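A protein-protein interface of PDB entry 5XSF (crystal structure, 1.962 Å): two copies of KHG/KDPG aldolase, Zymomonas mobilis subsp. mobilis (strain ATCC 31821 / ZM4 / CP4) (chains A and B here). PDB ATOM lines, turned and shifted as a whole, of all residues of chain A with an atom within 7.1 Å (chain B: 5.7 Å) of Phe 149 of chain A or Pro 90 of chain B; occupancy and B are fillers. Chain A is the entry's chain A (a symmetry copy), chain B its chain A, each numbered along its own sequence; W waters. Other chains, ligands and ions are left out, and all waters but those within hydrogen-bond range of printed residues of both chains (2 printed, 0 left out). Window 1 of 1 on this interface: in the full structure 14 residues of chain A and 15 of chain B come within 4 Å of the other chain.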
ATOM      1  N   ASN A 113       3.945   1.388  19.656  1.00  0.00           N
ATOM      2  CA  ASN A 113       3.475   0.693  20.843  1.00  0.00           C
ATOM      3  C   ASN A 113       2.116   0.084  20.535  1.00  0.00           C
ATOM      4  O   ASN A 113       1.535   0.323  19.474  1.00  0.00           O
ATOM      5  CB  ASN A 113       3.413   1.642  22.038  1.00  0.00           C
ATOM      6  CG  ASN A 113       2.774   2.953  21.683  1.00  0.00           C
ATOM      7  OD1 ASN A 113       1.670   2.992  21.133  1.00  0.00           O
ATOM      8  ND2 ASN A 113       3.483   4.045  21.948  1.00  0.00           N
ATOM      9  N   ALA A 114       1.617  -0.724  21.477  1.00  0.00           N
ATOM     10  CA  ALA A 114       0.426  -1.528  21.210  1.00  0.00           C
ATOM     11  C   ALA A 114      -0.806  -0.670  20.939  1.00  0.00           C
ATOM     12  O   ALA A 114      -1.667  -1.066  20.145  1.00  0.00           O
ATOM     13  CB  ALA A 114       0.159  -2.474  22.382  1.00  0.00           C
ATOM     14  N   ALA A 115      -0.913   0.498  21.577  1.00  0.00           N
ATOM     15  CA  ALA A 115      -2.066   1.355  21.328  1.00  0.00           C
ATOM     16  C   ALA A 115      -2.120   1.827  19.879  1.00  0.00           C
ATOM     17  O   ALA A 115      -3.213   1.983  19.322  1.00  0.00           O
ATOM     18  CB  ALA A 115      -2.050   2.556  22.276  1.00  0.00           C
ATOM     19  N   ASP A 116      -0.958   2.057  19.253  1.00  0.00           N
ATOM     20  CA  ASP A 116      -0.941   2.467  17.852  1.00  0.00           C
ATOM     21  C   ASP A 116      -1.434   1.346  16.948  1.00  0.00           C
ATOM     22  O   ASP A 116      -2.166   1.593  15.981  1.00  0.00           O
ATOM     23  CB  ASP A 116       0.470   2.878  17.423  1.00  0.00           C
ATOM     24  CG  ASP A 116       1.042   4.020  18.240  1.00  0.00           C
ATOM     25  OD1 ASP A 116       0.277   4.898  18.701  1.00  0.00           O
ATOM     26  OD2 ASP A 116       2.284   4.053  18.401  1.00  0.00           O
ATOM     27  N   VAL A 117      -1.035   0.107  17.242  1.00  0.00           N
ATOM     28  CA  VAL A 117      -1.483  -1.031  16.447  1.00  0.00           C
ATOM     29  C   VAL A 117      -2.988  -1.212  16.587  1.00  0.00           C
ATOM     30  O   VAL A 117      -3.694  -1.467  15.602  1.00  0.00           O
ATOM     31  CB  VAL A 117      -0.720  -2.301  16.868  1.00  0.00           C
ATOM     32  CG1 VAL A 117      -1.226  -3.515  16.104  1.00  0.00           C
ATOM     33  CG2 VAL A 117       0.778  -2.115  16.660  1.00  0.00           C
ATOM     34  N   MET A 118      -3.505  -1.066  17.811  1.00  0.00           N
ATOM     35  CA  MET A 118      -4.929  -1.284  18.034  1.00  0.00           C
ATOM     36  C   MET A 118      -5.774  -0.234  17.326  1.00  0.00           C
ATOM     37  O   MET A 118      -6.851  -0.550  16.805  1.00  0.00           O
ATOM     38  CB  MET A 118      -5.221  -1.302  19.534  1.00  0.00           C
ATOM     39  CG  MET A 118      -4.645  -2.525  20.242  1.00  0.00           C
ATOM     40  SD  MET A 118      -4.777  -2.431  22.030  1.00  0.00           S
ATOM     41  CE  MET A 118      -6.547  -2.276  22.237  1.00  0.00           C
ATOM     42  N   LEU A 121      -5.808  -1.396  13.732  1.00  0.00           N
ATOM     43  CA  LEU A 121      -6.712  -2.527  13.545  1.00  0.00           C
ATOM     44  C   LEU A 121      -8.163  -2.068  13.552  1.00  0.00           C
ATOM     45  O   LEU A 121      -8.984  -2.563  12.769  1.00  0.00           O
ATOM     46  CB  LEU A 121      -6.473  -3.575  14.631  1.00  0.00           C
ATOM     47  CG  LEU A 121      -5.118  -4.280  14.596  1.00  0.00           C
ATOM     48  CD1 LEU A 121      -4.897  -5.068  15.879  1.00  0.00           C
ATOM     49  CD2 LEU A 121      -5.025  -5.189  13.376  1.00  0.00           C
ATOM     50  N   PHE A 128       2.110  -2.202   9.226  1.00  0.00           N
ATOM     51  CA  PHE A 128       2.652  -0.985   9.820  1.00  0.00           C
ATOM     52  C   PHE A 128       4.171  -0.963   9.738  1.00  0.00           C
ATOM     53  O   PHE A 128       4.826  -2.009   9.742  1.00  0.00           O
ATOM     54  CB  PHE A 128       2.265  -0.836  11.305  1.00  0.00           C
ATOM     55  CG  PHE A 128       0.811  -1.066  11.581  1.00  0.00           C
ATOM     56  CD1 PHE A 128      -0.126  -0.091  11.296  1.00  0.00           C
ATOM     57  CD2 PHE A 128       0.379  -2.262  12.126  1.00  0.00           C
ATOM     58  CE1 PHE A 128      -1.469  -0.308  11.548  1.00  0.00           C
ATOM     59  CE2 PHE A 128      -0.962  -2.486  12.379  1.00  0.00           C
ATOM     60  CZ  PHE A 128      -1.888  -1.508  12.087  1.00  0.00           C
ATOM     61  N   LYS A 143       9.750  -8.202  18.371  1.00  0.00           N
ATOM     62  CA  LYS A 143       9.361  -9.591  18.586  1.00  0.00           C
ATOM     63  C   LYS A 143       8.229  -9.694  19.599  1.00  0.00           C
ATOM     64  O   LYS A 143       7.281 -10.461  19.399  1.00  0.00           O
ATOM     65  CB  LYS A 143      10.561 -10.421  19.046  1.00  0.00           C
ATOM     66  CG  LYS A 143      11.512 -10.824  17.933  1.00  0.00           C
ATOM     67  CD  LYS A 143      12.689 -11.642  18.457  1.00  0.00           C
ATOM     68  CE  LYS A 143      12.369 -13.129  18.546  1.00  0.00           C
ATOM     69  NZ  LYS A 143      11.423 -13.473  19.646  1.00  0.00           N
ATOM     70  N   SER A 144       8.296  -8.914  20.685  1.00  0.00           N
ATOM     71  CA  SER A 144       7.223  -8.968  21.673  1.00  0.00           C
ATOM     72  C   SER A 144       5.911  -8.481  21.080  1.00  0.00           C
ATOM     73  O   SER A 144       4.839  -8.999  21.412  1.00  0.00           O
ATOM     74  CB  SER A 144       7.578  -8.123  22.901  1.00  0.00           C
ATOM     75  OG  SER A 144       8.800  -8.533  23.487  1.00  0.00           O
ATOM     76  N   MET A 145       5.984  -7.488  20.190  1.00  0.00           N
ATOM     77  CA  MET A 145       4.780  -6.942  19.582  1.00  0.00           C
ATOM     78  C   MET A 145       4.193  -7.908  18.563  1.00  0.00           C
ATOM     79  O   MET A 145       2.973  -8.102  18.515  1.00  0.00           O
ATOM     80  CB  MET A 145       5.099  -5.592  18.936  1.00  0.00           C
ATOM     81  CG  MET A 145       3.965  -4.992  18.129  1.00  0.00           C
ATOM     82  SD  MET A 145       4.366  -3.331  17.548  1.00  0.00           S
ATOM     83  CE  MET A 145       4.298  -2.426  19.089  1.00  0.00           C
ATOM     84  N   ALA A 146       5.050  -8.528  17.748  1.00  0.00           N
ATOM     85  CA  ALA A 146       4.580  -9.498  16.765  1.00  0.00           C
ATOM     86  C   ALA A 146       4.015 -10.740  17.439  1.00  0.00           C
ATOM     87  O   ALA A 146       3.110 -11.384  16.893  1.00  0.00           O
ATOM     88  CB  ALA A 146       5.716  -9.869  15.813  1.00  0.00           C
ATOM     89  N   SER A 147       4.518 -11.073  18.630  1.00  0.00           N
ATOM     90  CA  SER A 147       3.977 -12.191  19.389  1.00  0.00           C
ATOM     91  C   SER A 147       2.553 -11.913  19.855  1.00  0.00           C
ATOM     92  O   SER A 147       1.729 -12.832  19.928  1.00  0.00           O
ATOM     93  CB  SER A 147       4.888 -12.483  20.580  1.00  0.00           C
ATOM     94  OG  SER A 147       4.427 -13.593  21.325  1.00  0.00           O
ATOM     95  N   VAL A 148       2.241 -10.651  20.148  1.00  0.00           N
ATOM     96  CA  VAL A 148       0.909 -10.296  20.623  1.00  0.00           C
ATOM     97  C   VAL A 148      -0.067 -10.164  19.462  1.00  0.00           C
ATOM     98  O   VAL A 148      -1.201 -10.647  19.535  1.00  0.00           O
ATOM     99  CB  VAL A 148       0.986  -8.999  21.447  1.00  0.00           C
ATOM    100  CG1 VAL A 148      -0.404  -8.523  21.822  1.00  0.00           C
ATOM    101  CG2 VAL A 148       1.839  -9.211  22.677  1.00  0.00           C
ATOM    102  N   PHE A 149       0.355  -9.505  18.382  1.00  0.00           N
ATOM    103  CA  PHE A 149      -0.513  -9.210  17.241  1.00  0.00           C
ATOM    104  C   PHE A 149      -0.177 -10.188  16.115  1.00  0.00           C
ATOM    105  O   PHE A 149       0.575  -9.884  15.185  1.00  0.00           O
ATOM    106  CB  PHE A 149      -0.343  -7.755  16.805  1.00  0.00           C
ATOM    107  CG  PHE A 149      -0.703  -6.753  17.869  1.00  0.00           C
ATOM    108  CD1 PHE A 149      -2.030  -6.447  18.130  1.00  0.00           C
ATOM    109  CD2 PHE A 149       0.285  -6.106  18.596  1.00  0.00           C
ATOM    110  CE1 PHE A 149      -2.368  -5.520  19.101  1.00  0.00           C
ATOM    111  CE2 PHE A 149      -0.044  -5.177  19.571  1.00  0.00           C
ATOM    112  CZ  PHE A 149      -1.375  -4.886  19.825  1.00  0.00           C
ATOM    113  N   ARG A 150      -0.767 -11.381  16.208  1.00  0.00           N
ATOM    114  CA  ARG A 150      -0.387 -12.482  15.329  1.00  0.00           C
ATOM    115  C   ARG A 150      -0.740 -12.216  13.870  1.00  0.00           C
ATOM    116  O   ARG A 150      -0.092 -12.765  12.971  1.00  0.00           O
ATOM    117  CB  ARG A 150      -1.053 -13.776  15.796  1.00  0.00           C
ATOM    118  CG  ARG A 150      -0.733 -14.160  17.228  1.00  0.00           C
ATOM    119  CD  ARG A 150       0.714 -14.611  17.382  1.00  0.00           C
ATOM    120  NE  ARG A 150       0.933 -15.272  18.666  1.00  0.00           N
ATOM    121  CZ  ARG A 150       0.660 -16.553  18.897  1.00  0.00           C
ATOM    122  NH1 ARG A 150       0.155 -17.309  17.930  1.00  0.00           N
ATOM    123  NH2 ARG A 150       0.885 -17.080  20.095  1.00  0.00           N
ATOM    124  N   GLN A 151      -1.773 -11.426  13.607  1.00  0.00           N
ATOM    125  CA  GLN A 151      -2.169 -11.188  12.228  1.00  0.00           C
ATOM    126  C   GLN A 151      -1.475  -9.988  11.595  1.00  0.00           C
ATOM    127  O   GLN A 151      -1.642  -9.760  10.394  1.00  0.00           O
ATOM    128  CB  GLN A 151      -3.690 -11.022  12.144  1.00  0.00           C
ATOM    129  CG  GLN A 151      -4.478 -12.158  12.819  1.00  0.00           C
ATOM    130  CD  GLN A 151      -3.879 -13.543  12.579  1.00  0.00           C
ATOM    131  OE1 GLN A 151      -3.505 -13.898  11.456  1.00  0.00           O
ATOM    132  NE2 GLN A 151      -3.791 -14.334  13.643  1.00  0.00           N
ATOM    133  N   VAL A 152      -0.712  -9.228  12.358  1.00  0.00           N
ATOM    134  CA  VAL A 152      -0.068  -8.012  11.875  1.00  0.00           C
ATOM    135  C   VAL A 152       1.302  -8.348  11.294  1.00  0.00           C
ATOM    136  O   VAL A 152       1.995  -9.252  11.770  1.00  0.00           O
ATOM    137  CB  VAL A 152       0.029  -6.976  13.017  1.00  0.00           C
ATOM    138  CG1 VAL A 152       0.732  -5.718  12.556  1.00  0.00           C
ATOM    139  CG2 VAL A 152      -1.363  -6.636  13.545  1.00  0.00           C
ATOM    140  N   ARG A 153       1.709  -7.602  10.263  1.00  0.00           N
ATOM    141  CA  ARG A 153       3.053  -7.707   9.707  1.00  0.00           C
ATOM    142  C   ARG A 153       3.694  -6.324   9.670  1.00  0.00           C
ATOM    143  O   ARG A 153       2.996  -5.308   9.609  1.00  0.00           O
ATOM    144  CB  ARG A 153       3.033  -8.327   8.307  1.00  0.00           C
ATOM    145  CG  ARG A 153       2.380  -9.700   8.249  1.00  0.00           C
ATOM    146  CD  ARG A 153       3.187 -10.744   9.004  1.00  0.00           C
ATOM    147  NE  ARG A 153       2.619 -12.081   8.830  1.00  0.00           N
ATOM    148  CZ  ARG A 153       1.699 -12.615   9.625  1.00  0.00           C
ATOM    149  NH1 ARG A 153       1.232 -11.932  10.662  1.00  0.00           N
ATOM    150  NH2 ARG A 153       1.241 -13.835   9.377  1.00  0.00           N
ATOM    151  N   PHE A 154       5.030  -6.290   9.692  1.00  0.00           N
ATOM    152  CA  PHE A 154       5.762  -5.067  10.008  1.00  0.00           C
ATOM    153  C   PHE A 154       6.863  -4.755   9.000  1.00  0.00           C
ATOM    154  O   PHE A 154       7.367  -5.633   8.290  1.00  0.00           O
ATOM    155  CB  PHE A 154       6.406  -5.139  11.399  1.00  0.00           C
ATOM    156  CG  PHE A 154       5.425  -5.336  12.513  1.00  0.00           C
ATOM    157  CD1 PHE A 154       5.045  -6.610  12.898  1.00  0.00           C
ATOM    158  CD2 PHE A 154       4.892  -4.244  13.181  1.00  0.00           C
ATOM    159  CE1 PHE A 154       4.142  -6.792  13.932  1.00  0.00           C
ATOM    160  CE2 PHE A 154       3.993  -4.415  14.212  1.00  0.00           C
ATOM    161  CZ  PHE A 154       3.617  -5.691  14.590  1.00  0.00           C
ATOM    162  N   SER A 173       7.256 -12.375  10.772  1.00  0.00           N
ATOM    163  CA  SER A 173       6.320 -11.260  10.862  1.00  0.00           C
ATOM    164  C   SER A 173       6.839  -9.990  10.199  1.00  0.00           C
ATOM    165  O   SER A 173       6.096  -9.005  10.131  1.00  0.00           O
ATOM    166  CB  SER A 173       5.983 -10.961  12.326  1.00  0.00           C
ATOM    167  OG  SER A 173       5.114 -11.947  12.862  1.00  0.00           O
ATOM    168  N   THR B  69      -5.209 -10.104  25.498  1.00  0.00           N
ATOM    169  CA  THR B  69      -5.157  -9.694  24.095  1.00  0.00           C
ATOM    170  C   THR B  69      -6.557  -9.358  23.586  1.00  0.00           C
ATOM    171  O   THR B  69      -6.951  -9.717  22.474  1.00  0.00           O
ATOM    172  CB  THR B  69      -4.481 -10.762  23.230  1.00  0.00           C
ATOM    173  OG1 THR B  69      -3.377 -11.319  23.951  1.00  0.00           O
ATOM    174  CG2 THR B  69      -3.936 -10.145  21.935  1.00  0.00           C
ATOM    175  N   VAL B  70      -7.324  -8.669  24.430  1.00  0.00           N
ATOM    176  CA  VAL B  70      -8.656  -8.182  24.082  1.00  0.00           C
ATOM    177  C   VAL B  70      -8.458  -6.886  23.301  1.00  0.00           C
ATOM    178  O   VAL B  70      -8.165  -5.840  23.881  1.00  0.00           O
ATOM    179  CB  VAL B  70      -9.526  -7.974  25.321  1.00  0.00           C
ATOM    180  CG1 VAL B  70     -10.828  -7.291  24.949  1.00  0.00           C
ATOM    181  CG2 VAL B  70      -9.795  -9.313  26.008  1.00  0.00           C
ATOM    182  N   LEU B  71      -8.585  -6.957  21.974  1.00  0.00           N
ATOM    183  CA  LEU B  71      -8.208  -5.842  21.115  1.00  0.00           C
ATOM    184  C   LEU B  71      -9.343  -4.873  20.810  1.00  0.00           C
ATOM    185  O   LEU B  71      -9.069  -3.748  20.376  1.00  0.00           O
ATOM    186  CB  LEU B  71      -7.637  -6.367  19.794  1.00  0.00           C
ATOM    187  CG  LEU B  71      -6.440  -7.307  19.929  1.00  0.00           C
ATOM    188  CD1 LEU B  71      -5.852  -7.615  18.561  1.00  0.00           C
ATOM    189  CD2 LEU B  71      -5.392  -6.703  20.859  1.00  0.00           C
ATOM    190  N   VAL B  88      -7.742  -8.150  29.814  1.00  0.00           N
ATOM    191  CA  VAL B  88      -6.429  -7.539  29.656  1.00  0.00           C
ATOM    192  C   VAL B  88      -6.224  -7.212  28.184  1.00  0.00           C
ATOM    193  O   VAL B  88      -6.610  -7.995  27.309  1.00  0.00           O
ATOM    194  CB  VAL B  88      -5.313  -8.472  30.170  1.00  0.00           C
ATOM    195  CG1 VAL B  88      -3.962  -7.802  30.040  1.00  0.00           C
ATOM    196  CG2 VAL B  88      -5.583  -8.888  31.622  1.00  0.00           C
ATOM    197  N   SER B  89      -5.627  -6.057  27.910  1.00  0.00           N
ATOM    198  CA  SER B  89      -5.276  -5.683  26.549  1.00  0.00           C
ATOM    199  C   SER B  89      -3.840  -5.185  26.502  1.00  0.00           C
ATOM    200  O   SER B  89      -3.347  -4.611  27.479  1.00  0.00           O
ATOM    201  CB  SER B  89      -6.221  -4.594  26.015  1.00  0.00           C
ATOM    202  OG  SER B  89      -6.169  -3.427  26.819  1.00  0.00           O
ATOM    203  N   PRO B  90      -3.133  -5.428  25.392  1.00  0.00           N
ATOM    204  CA  PRO B  90      -1.774  -4.876  25.246  1.00  0.00           C
ATOM    205  C   PRO B  90      -1.719  -3.361  25.275  1.00  0.00           C
ATOM    206  O   PRO B  90      -0.690  -2.795  25.662  1.00  0.00           O
ATOM    207  CB  PRO B  90      -1.312  -5.441  23.892  1.00  0.00           C
ATOM    208  CG  PRO B  90      -2.573  -5.696  23.140  1.00  0.00           C
ATOM    209  CD  PRO B  90      -3.565  -6.155  24.186  1.00  0.00           C
ATOM    210  N   GLY B  91      -2.778  -2.692  24.826  1.00  0.00           N
ATOM    211  CA  GLY B  91      -2.845  -1.244  24.793  1.00  0.00           C
ATOM    212  C   GLY B  91      -4.271  -0.786  25.025  1.00  0.00           C
ATOM    213  O   GLY B  91      -5.140  -1.609  25.320  1.00  0.00           O
ATOM    214  N   LEU B  92      -4.537   0.508  24.888  1.00  0.00           N
ATOM    215  CA  LEU B  92      -5.859   1.056  25.155  1.00  0.00           C
ATOM    216  C   LEU B  92      -6.309   1.921  23.990  1.00  0.00           C
ATOM    217  O   LEU B  92      -5.541   2.750  23.496  1.00  0.00           O
ATOM    218  CB  LEU B  92      -5.853   1.878  26.446  1.00  0.00           C
ATOM    219  CG  LEU B  92      -7.177   2.512  26.876  1.00  0.00           C
ATOM    220  CD1 LEU B  92      -8.230   1.443  27.091  1.00  0.00           C
ATOM    221  CD2 LEU B  92      -6.967   3.316  28.142  1.00  0.00           C
ATOM    222  N   PRO B 109      -6.002  -2.451  31.014  1.00  0.00           N
ATOM    223  CA  PRO B 109      -5.347  -2.164  29.736  1.00  0.00           C
ATOM    224  C   PRO B 109      -3.862  -1.877  29.884  1.00  0.00           C
ATOM    225  O   PRO B 109      -3.400  -1.327  30.887  1.00  0.00           O
ATOM    226  CB  PRO B 109      -6.098  -0.926  29.229  1.00  0.00           C
ATOM    227  CG  PRO B 109      -6.725  -0.304  30.452  1.00  0.00           C
ATOM    228  CD  PRO B 109      -6.564  -1.238  31.626  1.00  0.00           C
ATOM    229  N   GLY B 110      -3.115  -2.245  28.848  1.00  0.00           N
ATOM    230  CA  GLY B 110      -1.713  -1.905  28.802  1.00  0.00           C
ATOM    231  C   GLY B 110      -1.492  -0.447  28.448  1.00  0.00           C
ATOM    232  O   GLY B 110      -2.266   0.172  27.720  1.00  0.00           O
ATOM    233  N   VAL B 111      -0.402   0.100  28.976  1.00  0.00           N
ATOM    234  CA  VAL B 111       0.046   1.448  28.654  1.00  0.00           C
ATOM    235  C   VAL B 111       1.548   1.379  28.449  1.00  0.00           C
ATOM    236  O   VAL B 111       2.234   0.538  29.037  1.00  0.00           O
ATOM    237  CB  VAL B 111      -0.299   2.485  29.754  1.00  0.00           C
ATOM    238  CG1 VAL B 111      -1.817   2.574  29.976  1.00  0.00           C
ATOM    239  CG2 VAL B 111       0.421   2.154  31.052  1.00  0.00           C
ATOM    240  N   LYS B 129      -1.596  -2.322  32.994  1.00  0.00           N
ATOM    241  CA  LYS B 129      -0.345  -2.989  32.670  1.00  0.00           C
ATOM    242  C   LYS B 129       0.652  -1.997  32.087  1.00  0.00           C
ATOM    243  O   LYS B 129       0.291  -1.137  31.282  1.00  0.00           O
ATOM    244  CB  LYS B 129      -0.581  -4.110  31.662  1.00  0.00           C
ATOM    245  CG  LYS B 129      -0.838  -5.467  32.259  1.00  0.00           C
ATOM    246  CD  LYS B 129      -0.985  -6.485  31.141  1.00  0.00           C
ATOM    247  CE  LYS B 129      -0.249  -6.051  29.881  1.00  0.00           C
ATOM    248  NZ  LYS B 129      -0.845  -6.626  28.649  1.00  0.00           N
ATOM    249  N   PHE B 131       3.321  -2.269  29.608  1.00  0.00           N
ATOM    250  CA  PHE B 131       3.658  -3.300  28.640  1.00  0.00           C
ATOM    251  C   PHE B 131       4.189  -2.721  27.334  1.00  0.00           C
ATOM    252  O   PHE B 131       3.671  -1.700  26.856  1.00  0.00           O
ATOM    253  CB  PHE B 131       2.405  -4.144  28.357  1.00  0.00           C
ATOM    254  CG  PHE B 131       2.565  -5.103  27.222  1.00  0.00           C
ATOM    255  CD1 PHE B 131       3.082  -6.368  27.443  1.00  0.00           C
ATOM    256  CD2 PHE B 131       2.203  -4.745  25.934  1.00  0.00           C
ATOM    257  CE1 PHE B 131       3.242  -7.254  26.402  1.00  0.00           C
ATOM    258  CE2 PHE B 131       2.362  -5.624  24.887  1.00  0.00           C
ATOM    259  CZ  PHE B 131       2.882  -6.881  25.120  1.00  0.00           C
HETATM  260  O   HOH W   1      -7.749  -3.262  18.002  1.00  0.00           O
HETATM  261  O   HOH W   2       3.377  -1.236  23.529  1.00  0.00           O
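The backbone carbonyl oxygen (O) of Gly 91 of chain B is in hydrogen-bond range of the side-chain hydroxyl (OG) of Ser 89 of chain B, at 2.6 Å. O of Val 111 of chain B lies within hydrogen-bond range of N of Phe 131 of chain B. The backbone carbonyl oxygen (O) of Val 88 of chain B lies within hydrogen-bond range of the backbone NH (N) of Thr 69 of chain B, at 3.1 Å.
The side-chain sulfur of Met 118 of chain A is in hydrogen-bond range of the backbone NH of Gly 91 of chain B.
Among the printed residues, merely in contact across the chains: Ala 114 of chain A with Pro 90 of chain B, Ala 114 of chain A with Gly 91 of chain B, Ala 115 of chain A with Leu 92 of chain B, Met 118 of chain A with Leu 71 of chain B, Leu 121 of chain A with Leu 71 of chain B, Val 148 of chain A with Thr 69 of chain B, Val 148 of chain A with Pro 90 of chain B, Val 148 of chain A with Phe 131 of chain B, Phe 149 of chain A with Leu 71 of chain B and Phe 149 of chain A with Pro 90 of chain B.
Of the 21 printed residues of chain A, 6 touch a printed residue of chain B. Hydrophobic or aromatic side chains of chain A that line the printed part of chain B: Ala 114, Ala 115, Met 118, Leu 121, Val 148 and Phe 149. Of the 13 printed residues of chain B, 6 touch a printed residue of chain A. Hydrophobic or aromatic side chains of chain B within 4 Å of the printed part of chain A: Leu 71, Pro 90 and Phe 131. Along chain B the printed residues that touch a printed residue of chain A span positions 69 to 131. Among the printed residues, 11 pairs touch across the chains. Among the printed residues, no Asp or Glu carboxylate lies within 4 Å of a Lys or Arg side-chain nitrogen of the other chain.
Of chain B, only Leu 71 and Pro 90 come within 4 Å of Phe 149 of chain A. Of chain A, only Ala 114 (3.4 Å), Val 148 (3.8 Å) and Phe 149 (3.6 Å) come within 4 Å of Pro 90 of chain B. Of the printed residues of chain B, Ala 115 of chain A touches Leu 92 (3.7 Å). Of the printed residues of chain A, Thr 69 of chain B touches Val 148. Val 111 of chain B touches none of the printed residues of chain A. The nearest residue of chain B that does not touch Phe 149 of chain A is Thr 69 of chain B (5.6 Å). The nearest residue of chain A that does not touch Pro 90 of chain B is Met 118 of chain A (4.1 Å). The nearest printed residue of chain B that does not touch Leu 121 of chain A is Pro 90 of chain B (7.6 Å).
Water W2 lies within hydrogen-bond range of N of Ala 114 of chain A (2.8 Å) and O of Phe 131 of chain B (3.4 Å). Water W1 lies within hydrogen-bond range of the backbone carbonyl oxygen (O) of Leu 71 of chain B (2.8 Å) and the backbone carbonyl oxygen (O) of Met 118 of chain A (3.1 Å).
No position is printed for both chains. Of the 11 pairs that touch across the chains among the printed residues, none has its exchanged pair printed and touching as well.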
